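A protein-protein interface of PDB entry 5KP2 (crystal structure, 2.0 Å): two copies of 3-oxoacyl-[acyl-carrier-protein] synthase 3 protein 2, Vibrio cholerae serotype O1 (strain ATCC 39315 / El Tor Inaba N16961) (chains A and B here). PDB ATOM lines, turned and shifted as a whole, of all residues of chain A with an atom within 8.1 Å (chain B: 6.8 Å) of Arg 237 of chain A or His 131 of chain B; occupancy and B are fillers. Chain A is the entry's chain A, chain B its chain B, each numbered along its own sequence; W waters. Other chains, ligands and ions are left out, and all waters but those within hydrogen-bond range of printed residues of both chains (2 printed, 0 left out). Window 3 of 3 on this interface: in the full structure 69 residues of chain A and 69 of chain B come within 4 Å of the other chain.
The side-chain carboxylate of Glu 121 of chain A lies within hydrogen-bond range of the side-chain hydroxyl of Tyr 132 of chain B (2.6 Å).
The side-chain carboxylate (OD1) of Asp 178 of chain A is in hydrogen-bond range of a ring nitrogen (NE2) of His 131 of chain B (2.8 Å).
The backbone carbonyl oxygen (O) of Ala 179 of chain A sits at hydrogen-bond distance from a ring nitrogen (NE2) of His 131 of chain B, 3.1 Å away.
A ring nitrogen (NE2) of His 131 of chain B sits at hydrogen-bond distance from the guanidinium group (NH2) of Arg 237 of chain A (3.0 Å).
No position is printed for both chains.
Of the 10 pairs that touch across the chains among the printed residues, none has its exchanged pair printed and touching as well.
The guanidinium group (NE) of Arg 125 of chain A lies within salt-bridge range of the side-chain carboxylate (OE1) of Glu 121 of chain A, 2.8 Å away.
O of Gln 177 of chain A lies within hydrogen-bond range of NH2 of Arg 125 of chain A (2.8 Å).
The side-chain carboxylate of Asp 178 of chain A is in salt-bridge range of the guanidinium group of Arg 237 of chain A.
The backbone carbonyl oxygen (O) of Asp 178 of chain A sits at hydrogen-bond distance from the backbone NH (N) of His 321 of chain A (2.9 Å).
OE1 of Gln 233 of chain A sits at hydrogen-bond distance from NH1 of Arg 237 of chain A (3.3 Å).
O of Ser 130 of chain B lies within hydrogen-bond range of NZ of Lys 169 of chain B, 2.7 Å away.
Printed residues of chain B that touch a printed residue of chain A: Leu 126, Ala 129, Ser 130, His 131 and Tyr 132.
Hydrophobic or aromatic side chains of chain B within 4 Å of the printed part of chain A: Leu 126, Ala 129, His 131 and Tyr 132.
Printed residues of chain A that touch a printed residue of chain B: Glu 121, Arg 125, Asp 178, Ala 179, Ile 181 and Arg 237.
Along chain A the printed residues that touch a printed residue of chain B span positions 121 to 237.
Arg 237 of chain A touches just one residue of chain B: His 131.
Of the printed residues of chain A, His 131 of chain B touches Asp 178 (2.8 Å), Ala 179 (3.1 Å) and Arg 237 (3.0 Å).
Ser 130 of chain B touches just these residues of chain A: Glu 121 (3.9 Å) and Arg 125 (3.9 Å).
Printed residues of chain A within 4 Å of Tyr 132 of chain B: Glu 121 and Ile 181.
Printed residues of chain B within 4 Å of Glu 121 of chain A: Leu 126, Ser 130 and Tyr 132.
Printed residues of chain B within 4 Å of Arg 125 of chain A: Leu 126, Ala 129 and Ser 130.
Ser 238 of chain A touches none of the printed residues of chain B.
Leu 235 of chain A touches none of the printed residues of chain B.
The nearest printed residue of chain A that does not touch Ala 129 of chain B is Glu 121 of chain A (6.9 Å).
Among the printed residues, pairs that only touch across the chains: Glu 121 of chain A with Leu 126 of chain B, Glu 121 of chain A with Ser 130 of chain B, Arg 125 of chain A with Leu 126 of chain B, Arg 125 of chain A with Ala 129 of chain B, Arg 125 of chain A with Ser 130 of chain B and Ile 181 of chain A with Tyr 132 of chain B.
Water W1 lies within hydrogen-bond range of the side-chain hydroxyl (OG) of Ser 130 of chain B (2.5 Å), the side-chain carboxylate (OE2) of Glu 121 of chain A (2.8 Å), the guanidinium group (NH2) of Arg 125 of chain A (2.9 Å) and the backbone carbonyl oxygen (O) of Ala 179 of chain A (3.0 Å).
Water W2 bridges the side-chain hydroxyl of Tyr 132 of chain B (2.7 Å) and the backbone NH of Ile 181 of chain A (2.9 Å).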
ATOM      1  N   GLU A 121      34.975 -23.124 -17.423  1.00  0.00           N
ATOM      2  CA  GLU A 121      33.846 -24.036 -17.691  1.00  0.00           C
ATOM      3  C   GLU A 121      34.329 -25.231 -18.534  1.00  0.00           C
ATOM      4  O   GLU A 121      34.110 -26.376 -18.173  1.00  0.00           O
ATOM      5  CB  GLU A 121      32.717 -23.276 -18.387  1.00  0.00           C
ATOM      6  CG  GLU A 121      31.671 -24.082 -19.150  1.00  0.00           C
ATOM      7  CD  GLU A 121      30.653 -24.801 -18.289  1.00  0.00           C
ATOM      8  OE1 GLU A 121      30.860 -24.964 -17.075  1.00  0.00           O
ATOM      9  OE2 GLU A 121      29.606 -25.225 -18.849  1.00  0.00           O
ATOM     10  N   ARG A 125      34.581 -29.176 -17.223  1.00  0.00           N
ATOM     11  CA  ARG A 125      33.779 -30.246 -17.811  1.00  0.00           C
ATOM     12  C   ARG A 125      34.631 -31.311 -18.482  1.00  0.00           C
ATOM     13  O   ARG A 125      34.291 -32.497 -18.386  1.00  0.00           O
ATOM     14  CB  ARG A 125      32.728 -29.717 -18.802  1.00  0.00           C
ATOM     15  CG  ARG A 125      31.762 -28.678 -18.260  1.00  0.00           C
ATOM     16  CD  ARG A 125      31.302 -28.873 -16.843  1.00  0.00           C
ATOM     17  NE  ARG A 125      30.681 -27.663 -16.337  1.00  0.00           N
ATOM     18  CZ  ARG A 125      30.277 -27.483 -15.084  1.00  0.00           C
ATOM     19  NH1 ARG A 125      30.415 -28.443 -14.171  1.00  0.00           N
ATOM     20  NH2 ARG A 125      29.751 -26.316 -14.727  1.00  0.00           N
ATOM     21  N   GLN A 177      30.916 -25.070  -9.732  1.00  0.00           N
ATOM     22  CA  GLN A 177      29.687 -25.854  -9.619  1.00  0.00           C
ATOM     23  C   GLN A 177      28.849 -25.530 -10.870  1.00  0.00           C
ATOM     24  O   GLN A 177      29.265 -25.885 -11.955  1.00  0.00           O
ATOM     25  CB  GLN A 177      28.964 -25.543  -8.299  1.00  0.00           C
ATOM     26  CG  GLN A 177      29.809 -25.748  -7.047  1.00  0.00           C
ATOM     27  CD  GLN A 177      30.345 -27.165  -6.925  1.00  0.00           C
ATOM     28  OE1 GLN A 177      29.571 -28.107  -6.774  1.00  0.00           O
ATOM     29  NE2 GLN A 177      31.665 -27.329  -7.015  1.00  0.00           N
ATOM     30  N   ASP A 178      27.704 -24.855 -10.774  1.00  0.00           N
ATOM     31  CA  ASP A 178      26.995 -24.474 -11.993  1.00  0.00           C
ATOM     32  C   ASP A 178      27.655 -23.253 -12.665  1.00  0.00           C
ATOM     33  O   ASP A 178      28.264 -22.406 -12.007  1.00  0.00           O
ATOM     34  CB  ASP A 178      25.516 -24.207 -11.747  1.00  0.00           C
ATOM     35  CG  ASP A 178      24.743 -24.026 -13.044  1.00  0.00           C
ATOM     36  OD1 ASP A 178      24.957 -24.831 -14.001  1.00  0.00           O
ATOM     37  OD2 ASP A 178      23.930 -23.066 -13.141  1.00  0.00           O
ATOM     38  N   ALA A 179      27.540 -23.218 -13.991  1.00  0.00           N
ATOM     39  CA  ALA A 179      27.931 -22.091 -14.792  1.00  0.00           C
ATOM     40  C   ALA A 179      26.934 -21.925 -15.913  1.00  0.00           C
ATOM     41  O   ALA A 179      26.375 -22.903 -16.397  1.00  0.00           O
ATOM     42  CB  ALA A 179      29.318 -22.300 -15.376  1.00  0.00           C
ATOM     43  N   GLN A 180      26.718 -20.680 -16.319  1.00  0.00           N
ATOM     44  CA  GLN A 180      26.013 -20.410 -17.544  1.00  0.00           C
ATOM     45  C   GLN A 180      26.771 -19.386 -18.358  1.00  0.00           C
ATOM     46  O   GLN A 180      26.991 -18.258 -17.912  1.00  0.00           O
ATOM     47  CB  GLN A 180      24.588 -19.934 -17.314  1.00  0.00           C
ATOM     48  CG  GLN A 180      23.858 -19.901 -18.655  1.00  0.00           C
ATOM     49  CD  GLN A 180      22.424 -19.564 -18.524  1.00  0.00           C
ATOM     50  OE1 GLN A 180      22.083 -18.493 -18.006  1.00  0.00           O
ATOM     51  NE2 GLN A 180      21.552 -20.446 -19.017  1.00  0.00           N
ATOM     52  N   ILE A 181      27.122 -19.795 -19.576  1.00  0.00           N
ATOM     53  CA  ILE A 181      27.851 -18.973 -20.501  1.00  0.00           C
ATOM     54  C   ILE A 181      27.025 -18.824 -21.783  1.00  0.00           C
ATOM     55  O   ILE A 181      26.252 -19.688 -22.128  1.00  0.00           O
ATOM     56  CB  ILE A 181      29.263 -19.545 -20.781  1.00  0.00           C
ATOM     57  CG1 ILE A 181      29.215 -21.030 -21.194  1.00  0.00           C
ATOM     58  CG2 ILE A 181      30.129 -19.360 -19.545  1.00  0.00           C
ATOM     59  CD1 ILE A 181      30.488 -21.543 -21.843  1.00  0.00           C
ATOM     60  N   ALA A 229      21.247 -12.050 -15.881  1.00  0.00           N
ATOM     61  CA  ALA A 229      20.423 -13.239 -16.070  1.00  0.00           C
ATOM     62  C   ALA A 229      21.239 -14.540 -15.902  1.00  0.00           C
ATOM     63  O   ALA A 229      20.726 -15.533 -15.379  1.00  0.00           O
ATOM     64  CB  ALA A 229      19.714 -13.197 -17.423  1.00  0.00           C
ATOM     65  N   ALA A 230      22.500 -14.522 -16.334  1.00  0.00           N
ATOM     66  CA  ALA A 230      23.389 -15.678 -16.144  1.00  0.00           C
ATOM     67  C   ALA A 230      23.620 -15.947 -14.660  1.00  0.00           C
ATOM     68  O   ALA A 230      23.513 -17.080 -14.205  1.00  0.00           O
ATOM     69  CB  ALA A 230      24.714 -15.455 -16.848  1.00  0.00           C
ATOM     70  N   ALA A 231      23.904 -14.879 -13.909  1.00  0.00           N
ATOM     71  CA  ALA A 231      24.074 -14.988 -12.464  1.00  0.00           C
ATOM     72  C   ALA A 231      22.814 -15.552 -11.801  1.00  0.00           C
ATOM     73  O   ALA A 231      22.905 -16.434 -10.958  1.00  0.00           O
ATOM     74  CB  ALA A 231      24.461 -13.644 -11.874  1.00  0.00           C
ATOM     75  N   GLN A 232      21.640 -15.078 -12.221  1.00  0.00           N
ATOM     76  CA  GLN A 232      20.371 -15.601 -11.700  1.00  0.00           C
ATOM     77  C   GLN A 232      20.169 -17.096 -11.953  1.00  0.00           C
ATOM     78  O   GLN A 232      19.738 -17.825 -11.059  1.00  0.00           O
ATOM     79  CB  GLN A 232      19.172 -14.818 -12.265  1.00  0.00           C
ATOM     80  CG  GLN A 232      18.985 -13.425 -11.695  1.00  0.00           C
ATOM     81  CD  GLN A 232      18.958 -13.399 -10.168  1.00  0.00           C
ATOM     82  OE1 GLN A 232      19.736 -12.680  -9.554  1.00  0.00           O
ATOM     83  NE2 GLN A 232      18.114 -14.210  -9.561  1.00  0.00           N
ATOM     84  N   GLN A 233      20.463 -17.537 -13.166  1.00  0.00           N
ATOM     85  CA  GLN A 233      20.364 -18.961 -13.515  1.00  0.00           C
ATOM     86  C   GLN A 233      21.251 -19.830 -12.639  1.00  0.00           C
ATOM     87  O   GLN A 233      20.809 -20.837 -12.110  1.00  0.00           O
ATOM     88  CB  GLN A 233      20.716 -19.176 -14.982  1.00  0.00           C
ATOM     89  CG  GLN A 233      19.631 -18.686 -15.916  1.00  0.00           C
ATOM     90  CD  GLN A 233      18.555 -19.726 -16.102  1.00  0.00           C
ATOM     91  OE1 GLN A 233      18.787 -20.778 -16.726  1.00  0.00           O
ATOM     92  NE2 GLN A 233      17.364 -19.453 -15.567  1.00  0.00           N
ATOM     93  N   VAL A 234      22.497 -19.387 -12.474  1.00  0.00           N
ATOM     94  CA  VAL A 234      23.483 -20.066 -11.652  1.00  0.00           C
ATOM     95  C   VAL A 234      23.016 -20.149 -10.192  1.00  0.00           C
ATOM     96  O   VAL A 234      23.008 -21.221  -9.601  1.00  0.00           O
ATOM     97  CB  VAL A 234      24.855 -19.378 -11.813  1.00  0.00           C
ATOM     98  CG1 VAL A 234      25.824 -19.772 -10.721  1.00  0.00           C
ATOM     99  CG2 VAL A 234      25.437 -19.724 -13.188  1.00  0.00           C
ATOM    100  N   LEU A 235      22.628 -19.009  -9.635  1.00  0.00           N
ATOM    101  CA  LEU A 235      22.125 -18.955  -8.266  1.00  0.00           C
ATOM    102  C   LEU A 235      20.880 -19.819  -8.074  1.00  0.00           C
ATOM    103  O   LEU A 235      20.800 -20.594  -7.119  1.00  0.00           O
ATOM    104  CB  LEU A 235      21.832 -17.513  -7.876  1.00  0.00           C
ATOM    105  CG  LEU A 235      23.035 -16.596  -7.742  1.00  0.00           C
ATOM    106  CD1 LEU A 235      22.588 -15.157  -7.511  1.00  0.00           C
ATOM    107  CD2 LEU A 235      23.930 -17.067  -6.603  1.00  0.00           C
ATOM    108  N   ALA A 236      19.936 -19.713  -9.000  1.00  0.00           N
ATOM    109  CA  ALA A 236      18.721 -20.535  -8.961  1.00  0.00           C
ATOM    110  C   ALA A 236      19.015 -22.030  -9.031  1.00  0.00           C
ATOM    111  O   ALA A 236      18.427 -22.808  -8.279  1.00  0.00           O
ATOM    112  CB  ALA A 236      17.765 -20.130 -10.076  1.00  0.00           C
ATOM    113  N   ARG A 237      19.939 -22.438  -9.891  1.00  0.00           N
ATOM    114  CA  ARG A 237      20.346 -23.855  -9.954  1.00  0.00           C
ATOM    115  C   ARG A 237      21.099 -24.324  -8.702  1.00  0.00           C
ATOM    116  O   ARG A 237      20.985 -25.488  -8.309  1.00  0.00           O
ATOM    117  CB  ARG A 237      21.152 -24.182 -11.239  1.00  0.00           C
ATOM    118  CG  ARG A 237      20.252 -24.565 -12.419  1.00  0.00           C
ATOM    119  CD  ARG A 237      20.970 -25.330 -13.520  1.00  0.00           C
ATOM    120  NE  ARG A 237      21.842 -24.448 -14.293  1.00  0.00           N
ATOM    121  CZ  ARG A 237      21.453 -23.633 -15.278  1.00  0.00           C
ATOM    122  NH1 ARG A 237      20.187 -23.576 -15.694  1.00  0.00           N
ATOM    123  NH2 ARG A 237      22.363 -22.880 -15.885  1.00  0.00           N
ATOM    124  N   SER A 238      21.865 -23.426  -8.084  1.00  0.00           N
ATOM    125  CA  SER A 238      22.620 -23.766  -6.878  1.00  0.00           C
ATOM    126  C   SER A 238      21.709 -24.066  -5.690  1.00  0.00           C
ATOM    127  O   SER A 238      22.084 -24.830  -4.812  1.00  0.00           O
ATOM    128  CB  SER A 238      23.567 -22.629  -6.494  1.00  0.00           C
ATOM    129  OG  SER A 238      22.852 -21.534  -5.927  1.00  0.00           O
ATOM    130  N   GLY A 239      20.532 -23.438  -5.659  1.00  0.00           N
ATOM    131  CA  GLY A 239      19.638 -23.502  -4.510  1.00  0.00           C
ATOM    132  C   GLY A 239      20.060 -22.610  -3.359  1.00  0.00           C
ATOM    133  O   GLY A 239      19.512 -22.718  -2.267  1.00  0.00           O
ATOM    134  N   LEU A 240      21.017 -21.713  -3.596  1.00  0.00           N
ATOM    135  CA  LEU A 240      21.468 -20.775  -2.575  1.00  0.00           C
ATOM    136  C   LEU A 240      20.610 -19.511  -2.624  1.00  0.00           C
ATOM    137  O   LEU A 240      20.189 -19.073  -3.690  1.00  0.00           O
ATOM    138  CB  LEU A 240      22.935 -20.388  -2.796  1.00  0.00           C
ATOM    139  CG  LEU A 240      24.013 -21.470  -2.624  1.00  0.00           C
ATOM    140  CD1 LEU A 240      25.377 -20.836  -2.823  1.00  0.00           C
ATOM    141  CD2 LEU A 240      23.951 -22.170  -1.270  1.00  0.00           C
ATOM    142  N   ALA A 319      28.367 -16.373 -16.149  1.00  0.00           N
ATOM    143  CA  ALA A 319      28.469 -16.408 -14.708  1.00  0.00           C
ATOM    144  C   ALA A 319      28.774 -17.821 -14.242  1.00  0.00           C
ATOM    145  O   ALA A 319      28.446 -18.812 -14.900  1.00  0.00           O
ATOM    146  CB  ALA A 319      27.185 -15.896 -14.043  1.00  0.00           C
ATOM    147  N   HIS A 321      29.305 -20.208 -10.359  1.00  0.00           N
ATOM    148  CA  HIS A 321      29.350 -20.375  -8.911  1.00  0.00           C
ATOM    149  C   HIS A 321      30.532 -21.299  -8.561  1.00  0.00           C
ATOM    150  O   HIS A 321      30.563 -22.470  -8.971  1.00  0.00           O
ATOM    151  CB  HIS A 321      28.026 -20.946  -8.410  1.00  0.00           C
ATOM    152  CG  HIS A 321      28.085 -21.464  -7.016  1.00  0.00           C
ATOM    153  ND1 HIS A 321      27.471 -22.638  -6.634  1.00  0.00           N
ATOM    154  CD2 HIS A 321      28.701 -20.979  -5.911  1.00  0.00           C
ATOM    155  CE1 HIS A 321      27.734 -22.867  -5.358  1.00  0.00           C
ATOM    156  NE2 HIS A 321      28.478 -21.876  -4.898  1.00  0.00           N
ATOM    157  N   ASP B  75      22.645 -24.674 -28.158  1.00  0.00           N
ATOM    158  CA  ASP B  75      23.171 -24.137 -26.893  1.00  0.00           C
ATOM    159  C   ASP B  75      24.647 -23.772 -26.920  1.00  0.00           C
ATOM    160  O   ASP B  75      25.140 -23.105 -26.006  1.00  0.00           O
ATOM    161  CB  ASP B  75      22.960 -25.174 -25.780  1.00  0.00           C
ATOM    162  CG  ASP B  75      21.498 -25.511 -25.568  1.00  0.00           C
ATOM    163  OD1 ASP B  75      20.643 -24.620 -25.741  1.00  0.00           O
ATOM    164  OD2 ASP B  75      21.187 -26.690 -25.250  1.00  0.00           O
ATOM    165  N   LEU B 126      31.344 -31.096 -22.655  1.00  0.00           N
ATOM    166  CA  LEU B 126      30.436 -30.054 -22.146  1.00  0.00           C
ATOM    167  C   LEU B 126      29.016 -30.582 -22.034  1.00  0.00           C
ATOM    168  O   LEU B 126      28.349 -30.387 -21.015  1.00  0.00           O
ATOM    169  CB  LEU B 126      30.466 -28.798 -23.027  1.00  0.00           C
ATOM    170  CG  LEU B 126      31.673 -27.876 -22.862  1.00  0.00           C
ATOM    171  CD1 LEU B 126      31.755 -26.906 -24.035  1.00  0.00           C
ATOM    172  CD2 LEU B 126      31.620 -27.105 -21.550  1.00  0.00           C
ATOM    173  N   MET B 127      28.574 -31.272 -23.090  1.00  0.00           N
ATOM    174  CA  MET B 127      27.255 -31.873 -23.104  1.00  0.00           C
ATOM    175  C   MET B 127      27.112 -32.999 -22.066  1.00  0.00           C
ATOM    176  O   MET B 127      26.081 -33.110 -21.420  1.00  0.00           O
ATOM    177  CB  MET B 127      26.910 -32.361 -24.513  1.00  0.00           C
ATOM    178  CG  MET B 127      26.779 -31.214 -25.519  1.00  0.00           C
ATOM    179  SD  MET B 127      26.721 -31.709 -27.252  1.00  0.00           S
ATOM    180  CE  MET B 127      25.153 -32.591 -27.218  1.00  0.00           C
ATOM    181  N   GLN B 128      28.144 -33.820 -21.902  1.00  0.00           N
ATOM    182  CA  GLN B 128      28.100 -34.925 -20.945  1.00  0.00           C
ATOM    183  C   GLN B 128      28.090 -34.462 -19.468  1.00  0.00           C
ATOM    184  O   GLN B 128      27.418 -35.066 -18.646  1.00  0.00           O
ATOM    185  CB  GLN B 128      29.263 -35.878 -21.180  1.00  0.00           C
ATOM    186  CG  GLN B 128      29.103 -36.702 -22.437  1.00  0.00           C
ATOM    187  CD  GLN B 128      30.273 -37.631 -22.708  1.00  0.00           C
ATOM    188  OE1 GLN B 128      31.436 -37.248 -22.537  1.00  0.00           O
ATOM    189  NE2 GLN B 128      29.978 -38.844 -23.158  1.00  0.00           N
ATOM    190  N   ALA B 129      28.800 -33.378 -19.162  1.00  0.00           N
ATOM    191  CA  ALA B 129      28.978 -32.922 -17.780  1.00  0.00           C
ATOM    192  C   ALA B 129      28.079 -31.746 -17.386  1.00  0.00           C
ATOM    193  O   ALA B 129      27.997 -31.415 -16.208  1.00  0.00           O
ATOM    194  CB  ALA B 129      30.431 -32.559 -17.541  1.00  0.00           C
ATOM    195  N   SER B 130      27.397 -31.125 -18.345  1.00  0.00           N
ATOM    196  CA  SER B 130      26.576 -29.951 -18.042  1.00  0.00           C
ATOM    197  C   SER B 130      25.298 -29.910 -18.891  1.00  0.00           C
ATOM    198  O   SER B 130      24.915 -30.912 -19.497  1.00  0.00           O
ATOM    199  CB  SER B 130      27.412 -28.689 -18.233  1.00  0.00           C
ATOM    200  OG  SER B 130      26.787 -27.577 -17.569  1.00  0.00           O
ATOM    201  N   HIS B 131      24.672 -28.743 -18.949  1.00  0.00           N
ATOM    202  CA  HIS B 131      23.333 -28.550 -19.557  1.00  0.00           C
ATOM    203  C   HIS B 131      23.453 -27.897 -20.939  1.00  0.00           C
ATOM    204  O   HIS B 131      23.166 -26.702 -21.118  1.00  0.00           O
ATOM    205  CB  HIS B 131      22.442 -27.709 -18.625  1.00  0.00           C
ATOM    206  CG  HIS B 131      23.153 -26.554 -18.001  1.00  0.00           C
ATOM    207  ND1 HIS B 131      23.631 -25.489 -18.738  1.00  0.00           N
ATOM    208  CD2 HIS B 131      23.539 -26.331 -16.721  1.00  0.00           C
ATOM    209  CE1 HIS B 131      24.246 -24.639 -17.934  1.00  0.00           C
ATOM    210  NE2 HIS B 131      24.197 -25.123 -16.701  1.00  0.00           N
ATOM    211  N   TYR B 132      23.964 -28.658 -21.891  1.00  0.00           N
ATOM    212  CA  TYR B 132      23.961 -28.272 -23.292  1.00  0.00           C
ATOM    213  C   TYR B 132      23.274 -29.435 -24.004  1.00  0.00           C
ATOM    214  O   TYR B 132      23.715 -30.579 -23.868  1.00  0.00           O
ATOM    215  CB  TYR B 132      25.379 -28.055 -23.826  1.00  0.00           C
ATOM    216  CG  TYR B 132      26.196 -27.043 -23.055  1.00  0.00           C
ATOM    217  CD1 TYR B 132      26.178 -25.690 -23.397  1.00  0.00           C
ATOM    218  CD2 TYR B 132      26.950 -27.427 -21.963  1.00  0.00           C
ATOM    219  CE1 TYR B 132      26.912 -24.749 -22.683  1.00  0.00           C
ATOM    220  CE2 TYR B 132      27.690 -26.497 -21.240  1.00  0.00           C
ATOM    221  CZ  TYR B 132      27.663 -25.156 -21.607  1.00  0.00           C
ATOM    222  OH  TYR B 132      28.400 -24.247 -20.886  1.00  0.00           O
ATOM    223  N   ARG B 133      22.183 -29.149 -24.708  1.00  0.00           N
ATOM    224  CA  ARG B 133      21.333 -30.174 -25.346  1.00  0.00           C
ATOM    225  C   ARG B 133      21.764 -30.420 -26.794  1.00  0.00           C
ATOM    226  O   ARG B 133      21.734 -31.562 -27.281  1.00  0.00           O
ATOM    227  CB  ARG B 133      19.850 -29.730 -25.394  1.00  0.00           C
ATOM    228  CG  ARG B 133      19.251 -29.072 -24.145  1.00  0.00           C
ATOM    229  CD  ARG B 133      18.015 -28.210 -24.460  1.00  0.00           C
ATOM    230  NE  ARG B 133      18.327 -26.791 -24.763  1.00  0.00           N
ATOM    231  CZ  ARG B 133      17.458 -25.911 -25.289  1.00  0.00           C
ATOM    232  NH1 ARG B 133      16.208 -26.266 -25.580  1.00  0.00           N
ATOM    233  NH2 ARG B 133      17.838 -24.652 -25.535  1.00  0.00           N
ATOM    234  N   LYS B 169      22.179 -34.420 -27.598  1.00  0.00           N
ATOM    235  CA  LYS B 169      22.336 -35.193 -26.371  1.00  0.00           C
ATOM    236  C   LYS B 169      21.424 -36.411 -26.408  1.00  0.00           C
ATOM    237  O   LYS B 169      20.272 -36.295 -26.805  1.00  0.00           O
ATOM    238  CB  LYS B 169      21.997 -34.324 -25.166  1.00  0.00           C
ATOM    239  CG  LYS B 169      22.490 -34.858 -23.836  1.00  0.00           C
ATOM    240  CD  LYS B 169      22.433 -33.752 -22.793  1.00  0.00           C
ATOM    241  CE  LYS B 169      23.143 -34.106 -21.511  1.00  0.00           C
ATOM    242  NZ  LYS B 169      23.418 -32.874 -20.694  1.00  0.00           N
HETATM  243  O   HOH W   1      27.819 -25.493 -16.775  1.00  0.00           O
HETATM  244  O   HOH W   2      26.415 -22.587 -20.170  1.00  0.00           O
